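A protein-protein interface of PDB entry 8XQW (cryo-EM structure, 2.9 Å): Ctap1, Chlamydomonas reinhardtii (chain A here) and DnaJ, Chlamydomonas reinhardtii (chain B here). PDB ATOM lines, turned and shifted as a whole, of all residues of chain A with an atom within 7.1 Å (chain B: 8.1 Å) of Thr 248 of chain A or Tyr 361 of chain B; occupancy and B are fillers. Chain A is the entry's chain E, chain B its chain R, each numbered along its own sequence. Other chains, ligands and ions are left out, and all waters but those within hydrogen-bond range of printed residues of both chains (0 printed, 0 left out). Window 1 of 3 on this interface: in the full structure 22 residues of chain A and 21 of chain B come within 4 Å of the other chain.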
ATOM      1  N   ASN A 189     -13.369  31.267  38.961  1.00  0.00           N
ATOM      2  CA  ASN A 189     -13.882  31.220  37.599  1.00  0.00           C
ATOM      3  C   ASN A 189     -14.781  32.430  37.405  1.00  0.00           C
ATOM      4  O   ASN A 189     -15.927  32.432  37.858  1.00  0.00           O
ATOM      5  CB  ASN A 189     -14.634  29.914  37.372  1.00  0.00           C
ATOM      6  CG  ASN A 189     -15.327  29.860  36.042  1.00  0.00           C
ATOM      7  OD1 ASN A 189     -14.799  30.313  35.038  1.00  0.00           O
ATOM      8  ND2 ASN A 189     -16.516  29.289  36.026  1.00  0.00           N
ATOM      9  N   TRP A 190     -14.270  33.453  36.722  1.00  0.00           N
ATOM     10  CA  TRP A 190     -14.947  34.742  36.700  1.00  0.00           C
ATOM     11  C   TRP A 190     -16.300  34.708  36.014  1.00  0.00           C
ATOM     12  O   TRP A 190     -17.040  35.688  36.116  1.00  0.00           O
ATOM     13  CB  TRP A 190     -14.064  35.797  36.038  1.00  0.00           C
ATOM     14  CG  TRP A 190     -13.898  35.671  34.558  1.00  0.00           C
ATOM     15  CD1 TRP A 190     -12.875  35.063  33.903  1.00  0.00           C
ATOM     16  CD2 TRP A 190     -14.760  36.198  33.549  1.00  0.00           C
ATOM     17  NE1 TRP A 190     -13.052  35.167  32.550  1.00  0.00           N
ATOM     18  CE2 TRP A 190     -14.204  35.861  32.309  1.00  0.00           C
ATOM     19  CE3 TRP A 190     -15.952  36.919  33.576  1.00  0.00           C
ATOM     20  CZ2 TRP A 190     -14.799  36.213  31.110  1.00  0.00           C
ATOM     21  CZ3 TRP A 190     -16.538  37.266  32.388  1.00  0.00           C
ATOM     22  CH2 TRP A 190     -15.964  36.916  31.170  1.00  0.00           C
ATOM     23  N   THR A 191     -16.649  33.627  35.333  1.00  0.00           N
ATOM     24  CA  THR A 191     -17.948  33.523  34.692  1.00  0.00           C
ATOM     25  C   THR A 191     -18.977  32.819  35.557  1.00  0.00           C
ATOM     26  O   THR A 191     -20.082  32.554  35.079  1.00  0.00           O
ATOM     27  CB  THR A 191     -17.839  32.765  33.379  1.00  0.00           C
ATOM     28  OG1 THR A 191     -18.076  31.384  33.636  1.00  0.00           O
ATOM     29  CG2 THR A 191     -16.462  32.904  32.808  1.00  0.00           C
ATOM     30  N   SER A 192     -18.646  32.496  36.798  1.00  0.00           N
ATOM     31  CA  SER A 192     -19.551  31.741  37.644  1.00  0.00           C
ATOM     32  C   SER A 192     -20.255  32.664  38.625  1.00  0.00           C
ATOM     33  O   SER A 192     -19.857  33.807  38.839  1.00  0.00           O
ATOM     34  CB  SER A 192     -18.799  30.651  38.395  1.00  0.00           C
ATOM     35  OG  SER A 192     -17.649  31.181  39.014  1.00  0.00           O
ATOM     36  N   VAL A 245     -20.563  15.837  31.426  1.00  0.00           N
ATOM     37  CA  VAL A 245     -21.113  17.153  31.146  1.00  0.00           C
ATOM     38  C   VAL A 245     -20.261  17.806  30.073  1.00  0.00           C
ATOM     39  O   VAL A 245     -19.093  17.471  29.888  1.00  0.00           O
ATOM     40  CB  VAL A 245     -21.166  18.063  32.387  1.00  0.00           C
ATOM     41  CG1 VAL A 245     -21.895  17.391  33.507  1.00  0.00           C
ATOM     42  CG2 VAL A 245     -19.782  18.438  32.816  1.00  0.00           C
ATOM     43  N   GLN A 246     -20.860  18.750  29.362  1.00  0.00           N
ATOM     44  CA  GLN A 246     -20.099  19.505  28.387  1.00  0.00           C
ATOM     45  C   GLN A 246     -19.242  20.551  29.086  1.00  0.00           C
ATOM     46  O   GLN A 246     -19.364  20.794  30.284  1.00  0.00           O
ATOM     47  CB  GLN A 246     -21.023  20.166  27.380  1.00  0.00           C
ATOM     48  CG  GLN A 246     -21.790  19.189  26.561  1.00  0.00           C
ATOM     49  CD  GLN A 246     -22.687  19.869  25.586  1.00  0.00           C
ATOM     50  OE1 GLN A 246     -22.554  21.060  25.342  1.00  0.00           O
ATOM     51  NE2 GLN A 246     -23.617  19.124  25.018  1.00  0.00           N
ATOM     52  N   LEU A 247     -18.361  21.179  28.316  1.00  0.00           N
ATOM     53  CA  LEU A 247     -17.447  22.147  28.898  1.00  0.00           C
ATOM     54  C   LEU A 247     -18.128  23.453  29.253  1.00  0.00           C
ATOM     55  O   LEU A 247     -17.617  24.189  30.098  1.00  0.00           O
ATOM     56  CB  LEU A 247     -16.298  22.421  27.941  1.00  0.00           C
ATOM     57  CG  LEU A 247     -15.436  21.244  27.521  1.00  0.00           C
ATOM     58  CD1 LEU A 247     -14.556  21.667  26.393  1.00  0.00           C
ATOM     59  CD2 LEU A 247     -14.595  20.777  28.664  1.00  0.00           C
ATOM     60  N   THR A 248     -19.242  23.779  28.618  1.00  0.00           N
ATOM     61  CA  THR A 248     -19.925  25.042  28.877  1.00  0.00           C
ATOM     62  C   THR A 248     -21.071  24.838  29.863  1.00  0.00           C
ATOM     63  O   THR A 248     -22.207  25.210  29.607  1.00  0.00           O
ATOM     64  CB  THR A 248     -20.442  25.630  27.574  1.00  0.00           C
ATOM     65  OG1 THR A 248     -21.763  25.140  27.336  1.00  0.00           O
ATOM     66  CG2 THR A 248     -19.562  25.209  26.421  1.00  0.00           C
ATOM     67  N   GLU A 249     -20.763  24.256  31.012  1.00  0.00           N
ATOM     68  CA  GLU A 249     -21.791  23.798  31.936  1.00  0.00           C
ATOM     69  C   GLU A 249     -21.504  24.329  33.329  1.00  0.00           C
ATOM     70  O   GLU A 249     -20.394  24.172  33.839  1.00  0.00           O
ATOM     71  CB  GLU A 249     -21.858  22.280  31.952  1.00  0.00           C
ATOM     72  CG  GLU A 249     -23.243  21.740  32.139  1.00  0.00           C
ATOM     73  CD  GLU A 249     -23.664  21.739  33.582  1.00  0.00           C
ATOM     74  OE1 GLU A 249     -24.858  21.509  33.862  1.00  0.00           O
ATOM     75  OE2 GLU A 249     -22.797  21.971  34.443  1.00  0.00           O
ATOM     76  N   GLN A 250     -22.512  24.934  33.951  1.00  0.00           N
ATOM     77  CA  GLN A 250     -22.419  25.466  35.308  1.00  0.00           C
ATOM     78  C   GLN A 250     -23.619  24.974  36.100  1.00  0.00           C
ATOM     79  O   GLN A 250     -24.639  25.655  36.183  1.00  0.00           O
ATOM     80  CB  GLN A 250     -22.365  26.945  35.290  1.00  0.00           C
ATOM     81  CG  GLN A 250     -21.274  27.505  34.439  1.00  0.00           C
ATOM     82  CD  GLN A 250     -21.595  28.884  33.958  1.00  0.00           C
ATOM     83  OE1 GLN A 250     -20.726  29.744  33.876  1.00  0.00           O
ATOM     84  NE2 GLN A 250     -22.855  29.108  33.631  1.00  0.00           N
ATOM     85  N   ALA A 266     -14.409  21.079  33.029  1.00  0.00           N
ATOM     86  CA  ALA A 266     -15.319  22.161  32.679  1.00  0.00           C
ATOM     87  C   ALA A 266     -14.908  23.459  33.355  1.00  0.00           C
ATOM     88  O   ALA A 266     -14.849  24.516  32.717  1.00  0.00           O
ATOM     89  CB  ALA A 266     -16.745  21.793  33.063  1.00  0.00           C
ATOM     90  N   TYR A 269     -11.761  24.901  31.890  1.00  0.00           N
ATOM     91  CA  TYR A 269     -11.965  25.470  30.566  1.00  0.00           C
ATOM     92  C   TYR A 269     -12.665  26.812  30.648  1.00  0.00           C
ATOM     93  O   TYR A 269     -12.350  27.730  29.889  1.00  0.00           O
ATOM     94  CB  TYR A 269     -12.769  24.505  29.709  1.00  0.00           C
ATOM     95  CG  TYR A 269     -13.289  25.076  28.418  1.00  0.00           C
ATOM     96  CD1 TYR A 269     -12.538  25.013  27.264  1.00  0.00           C
ATOM     97  CD2 TYR A 269     -14.547  25.639  28.343  1.00  0.00           C
ATOM     98  CE1 TYR A 269     -13.006  25.515  26.087  1.00  0.00           C
ATOM     99  CE2 TYR A 269     -15.024  26.144  27.168  1.00  0.00           C
ATOM    100  CZ  TYR A 269     -14.250  26.074  26.042  1.00  0.00           C
ATOM    101  OH  TYR A 269     -14.717  26.574  24.856  1.00  0.00           O
ATOM    102  N   GLN A 270     -13.622  26.948  31.560  1.00  0.00           N
ATOM    103  CA  GLN A 270     -14.361  28.199  31.645  1.00  0.00           C
ATOM    104  C   GLN A 270     -13.578  29.295  32.343  1.00  0.00           C
ATOM    105  O   GLN A 270     -13.865  30.475  32.135  1.00  0.00           O
ATOM    106  CB  GLN A 270     -15.679  27.986  32.373  1.00  0.00           C
ATOM    107  CG  GLN A 270     -16.552  26.951  31.758  1.00  0.00           C
ATOM    108  CD  GLN A 270     -17.711  26.609  32.635  1.00  0.00           C
ATOM    109  OE1 GLN A 270     -18.242  25.512  32.575  1.00  0.00           O
ATOM    110  NE2 GLN A 270     -18.110  27.546  33.466  1.00  0.00           N
ATOM    111  N   ALA A 271     -12.611  28.943  33.186  1.00  0.00           N
ATOM    112  CA  ALA A 271     -11.887  29.974  33.912  1.00  0.00           C
ATOM    113  C   ALA A 271     -11.048  30.851  33.003  1.00  0.00           C
ATOM    114  O   ALA A 271     -10.768  31.994  33.363  1.00  0.00           O
ATOM    115  CB  ALA A 271     -10.993  29.343  34.973  1.00  0.00           C
ATOM    116  N   GLU A 273     -11.706  32.198  30.097  1.00  0.00           N
ATOM    117  CA  GLU A 273     -12.438  32.946  29.094  1.00  0.00           C
ATOM    118  C   GLU A 273     -11.978  34.400  29.088  1.00  0.00           C
ATOM    119  O   GLU A 273     -11.867  35.020  30.148  1.00  0.00           O
ATOM    120  CB  GLU A 273     -13.931  32.876  29.372  1.00  0.00           C
ATOM    121  CG  GLU A 273     -14.779  33.447  28.277  1.00  0.00           C
ATOM    122  CD  GLU A 273     -14.683  32.644  27.008  1.00  0.00           C
ATOM    123  OE1 GLU A 273     -14.929  33.215  25.925  1.00  0.00           O
ATOM    124  OE2 GLU A 273     -14.359  31.442  27.091  1.00  0.00           O
ATOM    125  N   ASN B 345     -27.837  19.327  27.133  1.00  0.00           N
ATOM    126  CA  ASN B 345     -28.512  20.542  27.583  1.00  0.00           C
ATOM    127  C   ASN B 345     -27.726  21.142  28.734  1.00  0.00           C
ATOM    128  O   ASN B 345     -28.127  21.033  29.897  1.00  0.00           O
ATOM    129  CB  ASN B 345     -29.949  20.253  28.000  1.00  0.00           C
ATOM    130  CG  ASN B 345     -30.776  19.722  26.864  1.00  0.00           C
ATOM    131  OD1 ASN B 345     -30.920  20.372  25.834  1.00  0.00           O
ATOM    132  ND2 ASN B 345     -31.321  18.531  27.038  1.00  0.00           N
ATOM    133  N   PRO B 346     -26.610  21.793  28.448  1.00  0.00           N
ATOM    134  CA  PRO B 346     -25.861  22.451  29.514  1.00  0.00           C
ATOM    135  C   PRO B 346     -26.628  23.649  30.035  1.00  0.00           C
ATOM    136  O   PRO B 346     -27.249  24.397  29.276  1.00  0.00           O
ATOM    137  CB  PRO B 346     -24.564  22.871  28.825  1.00  0.00           C
ATOM    138  CG  PRO B 346     -24.944  23.050  27.424  1.00  0.00           C
ATOM    139  CD  PRO B 346     -26.037  22.074  27.124  1.00  0.00           C
ATOM    140  N   THR B 347     -26.583  23.825  31.349  1.00  0.00           N
ATOM    141  CA  THR B 347     -27.374  24.833  32.035  1.00  0.00           C
ATOM    142  C   THR B 347     -26.500  26.016  32.417  1.00  0.00           C
ATOM    143  O   THR B 347     -25.343  25.847  32.807  1.00  0.00           O
ATOM    144  CB  THR B 347     -28.030  24.243  33.283  1.00  0.00           C
ATOM    145  OG1 THR B 347     -28.861  23.140  32.904  1.00  0.00           O
ATOM    146  CG2 THR B 347     -28.882  25.275  33.988  1.00  0.00           C
ATOM    147  N   GLN B 348     -27.060  27.216  32.291  1.00  0.00           N
ATOM    148  CA  GLN B 348     -26.402  28.452  32.690  1.00  0.00           C
ATOM    149  C   GLN B 348     -27.080  28.983  33.945  1.00  0.00           C
ATOM    150  O   GLN B 348     -28.245  29.389  33.896  1.00  0.00           O
ATOM    151  CB  GLN B 348     -26.471  29.480  31.563  1.00  0.00           C
ATOM    152  CG  GLN B 348     -25.846  30.819  31.883  1.00  0.00           C
ATOM    153  CD  GLN B 348     -24.359  30.838  31.625  1.00  0.00           C
ATOM    154  OE1 GLN B 348     -23.765  29.816  31.286  1.00  0.00           O
ATOM    155  NE2 GLN B 348     -23.746  32.005  31.779  1.00  0.00           N
ATOM    156  N   VAL B 349     -26.360  28.980  35.067  1.00  0.00           N
ATOM    157  CA  VAL B 349     -26.930  29.459  36.322  1.00  0.00           C
ATOM    158  C   VAL B 349     -26.619  30.938  36.497  1.00  0.00           C
ATOM    159  O   VAL B 349     -27.471  31.713  36.939  1.00  0.00           O
ATOM    160  CB  VAL B 349     -26.425  28.651  37.530  1.00  0.00           C
ATOM    161  CG1 VAL B 349     -27.070  27.284  37.556  1.00  0.00           C
ATOM    162  CG2 VAL B 349     -24.918  28.533  37.505  1.00  0.00           C
ATOM    163  N   ALA B 350     -25.399  31.340  36.158  1.00  0.00           N
ATOM    164  CA  ALA B 350     -25.044  32.743  36.237  1.00  0.00           C
ATOM    165  C   ALA B 350     -25.855  33.544  35.228  1.00  0.00           C
ATOM    166  O   ALA B 350     -26.462  33.002  34.305  1.00  0.00           O
ATOM    167  CB  ALA B 350     -23.552  32.937  35.986  1.00  0.00           C
ATOM    168  N   THR B 355     -22.072  38.984  36.040  1.00  0.00           N
ATOM    169  CA  THR B 355     -20.769  38.731  35.445  1.00  0.00           C
ATOM    170  C   THR B 355     -20.749  39.323  34.044  1.00  0.00           C
ATOM    171  O   THR B 355     -21.563  38.945  33.195  1.00  0.00           O
ATOM    172  CB  THR B 355     -20.484  37.235  35.407  1.00  0.00           C
ATOM    173  OG1 THR B 355     -21.691  36.534  35.098  1.00  0.00           O
ATOM    174  CG2 THR B 355     -19.982  36.762  36.752  1.00  0.00           C
ATOM    175  N   GLN B 357     -20.146  39.047  31.105  1.00  0.00           N
ATOM    176  CA  GLN B 357     -19.855  38.126  30.015  1.00  0.00           C
ATOM    177  C   GLN B 357     -20.841  38.392  28.885  1.00  0.00           C
ATOM    178  O   GLN B 357     -22.029  38.074  29.002  1.00  0.00           O
ATOM    179  CB  GLN B 357     -19.940  36.683  30.494  1.00  0.00           C
ATOM    180  CG  GLN B 357     -19.453  35.681  29.484  1.00  0.00           C
ATOM    181  CD  GLN B 357     -20.032  34.311  29.714  1.00  0.00           C
ATOM    182  OE1 GLN B 357     -20.816  34.104  30.637  1.00  0.00           O
ATOM    183  NE2 GLN B 357     -19.653  33.365  28.872  1.00  0.00           N
ATOM    184  N   LEU B 358     -20.350  38.966  27.791  1.00  0.00           N
ATOM    185  CA  LEU B 358     -21.211  39.371  26.689  1.00  0.00           C
ATOM    186  C   LEU B 358     -21.323  38.326  25.593  1.00  0.00           C
ATOM    187  O   LEU B 358     -22.343  38.279  24.900  1.00  0.00           O
ATOM    188  CB  LEU B 358     -20.701  40.677  26.076  1.00  0.00           C
ATOM    189  CG  LEU B 358     -20.627  41.901  26.988  1.00  0.00           C
ATOM    190  CD1 LEU B 358     -20.648  43.171  26.157  1.00  0.00           C
ATOM    191  CD2 LEU B 358     -21.754  41.908  28.008  1.00  0.00           C
ATOM    192  N   LEU B 359     -20.320  37.504  25.417  1.00  0.00           N
ATOM    193  CA  LEU B 359     -20.292  36.526  24.347  1.00  0.00           C
ATOM    194  C   LEU B 359     -20.347  35.118  24.904  1.00  0.00           C
ATOM    195  O   LEU B 359     -19.876  34.857  26.014  1.00  0.00           O
ATOM    196  CB  LEU B 359     -19.021  36.695  23.517  1.00  0.00           C
ATOM    197  CG  LEU B 359     -18.742  38.115  23.044  1.00  0.00           C
ATOM    198  CD1 LEU B 359     -17.361  38.211  22.445  1.00  0.00           C
ATOM    199  CD2 LEU B 359     -19.786  38.505  22.026  1.00  0.00           C
ATOM    200  N   PRO B 360     -20.914  34.177  24.159  1.00  0.00           N
ATOM    201  CA  PRO B 360     -20.808  32.771  24.550  1.00  0.00           C
ATOM    202  C   PRO B 360     -19.357  32.323  24.553  1.00  0.00           C
ATOM    203  O   PRO B 360     -18.466  32.996  24.034  1.00  0.00           O
ATOM    204  CB  PRO B 360     -21.618  32.039  23.478  1.00  0.00           C
ATOM    205  CG  PRO B 360     -21.650  32.975  22.326  1.00  0.00           C
ATOM    206  CD  PRO B 360     -21.683  34.344  22.918  1.00  0.00           C
ATOM    207  N   TYR B 361     -19.124  31.162  25.154  1.00  0.00           N
ATOM    208  CA  TYR B 361     -17.765  30.666  25.280  1.00  0.00           C
ATOM    209  C   TYR B 361     -17.164  30.401  23.908  1.00  0.00           C
ATOM    210  O   TYR B 361     -17.871  30.290  22.906  1.00  0.00           O
ATOM    211  CB  TYR B 361     -17.739  29.395  26.118  1.00  0.00           C
ATOM    212  CG  TYR B 361     -18.235  29.584  27.527  1.00  0.00           C
ATOM    213  CD1 TYR B 361     -17.383  29.988  28.532  1.00  0.00           C
ATOM    214  CD2 TYR B 361     -19.556  29.350  27.851  1.00  0.00           C
ATOM    215  CE1 TYR B 361     -17.833  30.157  29.812  1.00  0.00           C
ATOM    216  CE2 TYR B 361     -20.012  29.515  29.131  1.00  0.00           C
ATOM    217  CZ  TYR B 361     -19.146  29.918  30.104  1.00  0.00           C
ATOM    218  OH  TYR B 361     -19.604  30.079  31.384  1.00  0.00           O
ATOM    219  N   GLY B 362     -15.849  30.311  23.870  1.00  0.00           N
ATOM    220  CA  GLY B 362     -15.109  30.097  22.651  1.00  0.00           C
ATOM    221  C   GLY B 362     -14.028  31.138  22.516  1.00  0.00           C
ATOM    222  O   GLY B 362     -13.880  32.020  23.358  1.00  0.00           O
ATOM    223  N   GLU B 363     -13.260  31.037  21.439  1.00  0.00           N
ATOM    224  CA  GLU B 363     -12.182  31.971  21.163  1.00  0.00           C
ATOM    225  C   GLU B 363     -12.493  32.770  19.910  1.00  0.00           C
ATOM    226  O   GLU B 363     -13.204  32.303  19.017  1.00  0.00           O
ATOM    227  CB  GLU B 363     -10.847  31.250  20.984  1.00  0.00           C
ATOM    228  CG  GLU B 363     -10.285  30.674  22.259  1.00  0.00           C
ATOM    229  CD  GLU B 363      -9.607  31.717  23.117  1.00  0.00           C
ATOM    230  OE1 GLU B 363      -9.091  31.355  24.190  1.00  0.00           O
ATOM    231  OE2 GLU B 363      -9.582  32.899  22.723  1.00  0.00           O
ATOM    232  N   GLY B 364     -11.943  33.980  19.851  1.00  0.00           N
ATOM    233  CA  GLY B 364     -12.136  34.852  18.711  1.00  0.00           C
ATOM    234  C   GLY B 364     -13.596  35.091  18.398  1.00  0.00           C
ATOM    235  O   GLY B 364     -14.038  34.887  17.263  1.00  0.00           O
ATOM    236  N   GLY B 365     -14.359  35.515  19.404  1.00  0.00           N
ATOM    237  CA  GLY B 365     -15.780  35.728  19.198  1.00  0.00           C
ATOM    238  C   GLY B 365     -16.081  36.999  18.426  1.00  0.00           C
ATOM    239  O   GLY B 365     -17.150  37.132  17.829  1.00  0.00           O
ATOM    240  N   ARG B 368     -16.155  36.436  14.834  1.00  0.00           N
ATOM    241  CA  ARG B 368     -17.334  35.598  14.661  1.00  0.00           C
ATOM    242  C   ARG B 368     -18.621  36.408  14.760  1.00  0.00           C
ATOM    243  O   ARG B 368     -19.671  35.960  14.286  1.00  0.00           O
ATOM    244  CB  ARG B 368     -17.332  34.484  15.707  1.00  0.00           C
ATOM    245  CG  ARG B 368     -16.718  33.184  15.237  1.00  0.00           C
ATOM    246  CD  ARG B 368     -17.745  32.320  14.533  1.00  0.00           C
ATOM    247  NE  ARG B 368     -18.894  32.033  15.388  1.00  0.00           N
ATOM    248  CZ  ARG B 368     -20.079  32.624  15.272  1.00  0.00           C
ATOM    249  NH1 ARG B 368     -21.067  32.302  16.095  1.00  0.00           N
ATOM    250  NH2 ARG B 368     -20.274  33.540  14.334  1.00  0.00           N
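The backbone carbonyl oxygen (O) of Asn 189 of chain A is in hydrogen-bond range of the side-chain hydroxyl (OG) of Ser 192 of chain A (2.4 Å).
The backbone carbonyl oxygen (O) of Leu 247 of chain A sits close to the side-chain amide oxygen (OE1) of Gln 270 of chain A (2.9 Å).
NE1 of Trp 190 of chain A lies within hydrogen-bond range of O of Glu 273 of chain A, at 2.7 Å.
The side-chain amide nitrogen (NE2) of Gln 357 of chain B sits at hydrogen-bond distance from the backbone carbonyl oxygen (O) of Leu 359 of chain B (3.2 Å).
O of Gln 270 of chain A lies close to OD1 of Asn 189 of chain A, 3.1 Å away.
O of Thr 191 of chain A lies close to OE1 of Gln 250 of chain A, 3.1 Å away.
Thr 355 of chain B touches Trp 190 of chain A (CG2 to O, 3.2 Å).
Trp 190 of chain A touches Gln 357 of chain B (CZ3 to CB, 3.9 Å).
Ser 192 of chain A touches Thr 355 of chain B.
Thr 248 of chain A touches Pro 346 of chain B.
Thr 248 of chain A touches Tyr 361 of chain B (CB to CD2, 3.8 Å).
CG of Glu 249 of chain A touches CB of Pro 346 of chain B (3.7 Å).
Glu 249 of chain A touches Thr 347 of chain B (OE1 to N, 3.8 Å).
Gln 250 of chain A touches Val 349 of chain B.
Gln 270 of chain A touches Tyr 361 of chain B (NE2 to OH, 3.6 Å).
Glu 273 of chain A touches Tyr 361 of chain B (OE2 to CD1, 3.7 Å).
Of the 15 printed residues of chain A, 9 touch a printed residue of chain B.
Of the 17 printed residues of chain B, 9 touch a printed residue of chain A.
Among the printed residues, no Asp or Glu carboxylate lies within 4 Å of a Lys or Arg side-chain nitrogen of the other chain.
The side-chain hydroxyl of Thr 191 of chain A sits at hydrogen-bond distance from the side-chain hydroxyl of Tyr 361 of chain B, 3.0 Å away.
The backbone carbonyl oxygen of Gly 362 of chain B lies close to the side-chain carboxylate of Glu 273 of chain A.
O of Thr 347 of chain B lies within hydrogen-bond range of N of Gln 250 of chain A (3.2 Å).
The side-chain hydroxyl of Tyr 361 of chain B sits at hydrogen-bond distance from the side-chain amide oxygen of Gln 250 of chain A (2.8 Å).
The side-chain amide oxygen of Gln 348 of chain B lies within hydrogen-bond range of the side-chain amide nitrogen of Gln 250 of chain A (2.6 Å).
Of the printed residues of chain B, Trp 190 of chain A touches Thr 355 (3.2 Å) and Gln 357 (3.9 Å).
Printed residues of chain B within 4 Å of Thr 191 of chain A: Ala 350 (3.6 Å) and Tyr 361 (3.0 Å).
Of chain B, only Pro 346 and Tyr 361 come within 4 Å of Thr 248 of chain A.
Of the printed residues of chain B, Glu 273 of chain A touches Tyr 361 (3.7 Å) and Gly 362 (3.0 Å).
Of the printed residues of chain A, Ala 350 of chain B touches Thr 191 (3.6 Å).
Leu 358 of chain B touches none of the printed residues of chain A.
Tyr 361 of chain B touches five residues of chain A.
Arg 368 of chain B touches none of the printed residues of chain A.
The nearest residue of chain A that does not touch Tyr 361 of chain B is Tyr 269 of chain A (4.3 Å).
The nearest printed residue of chain A that does not touch Gly 362 of chain B is Tyr 269 of chain A (4.03 Å).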
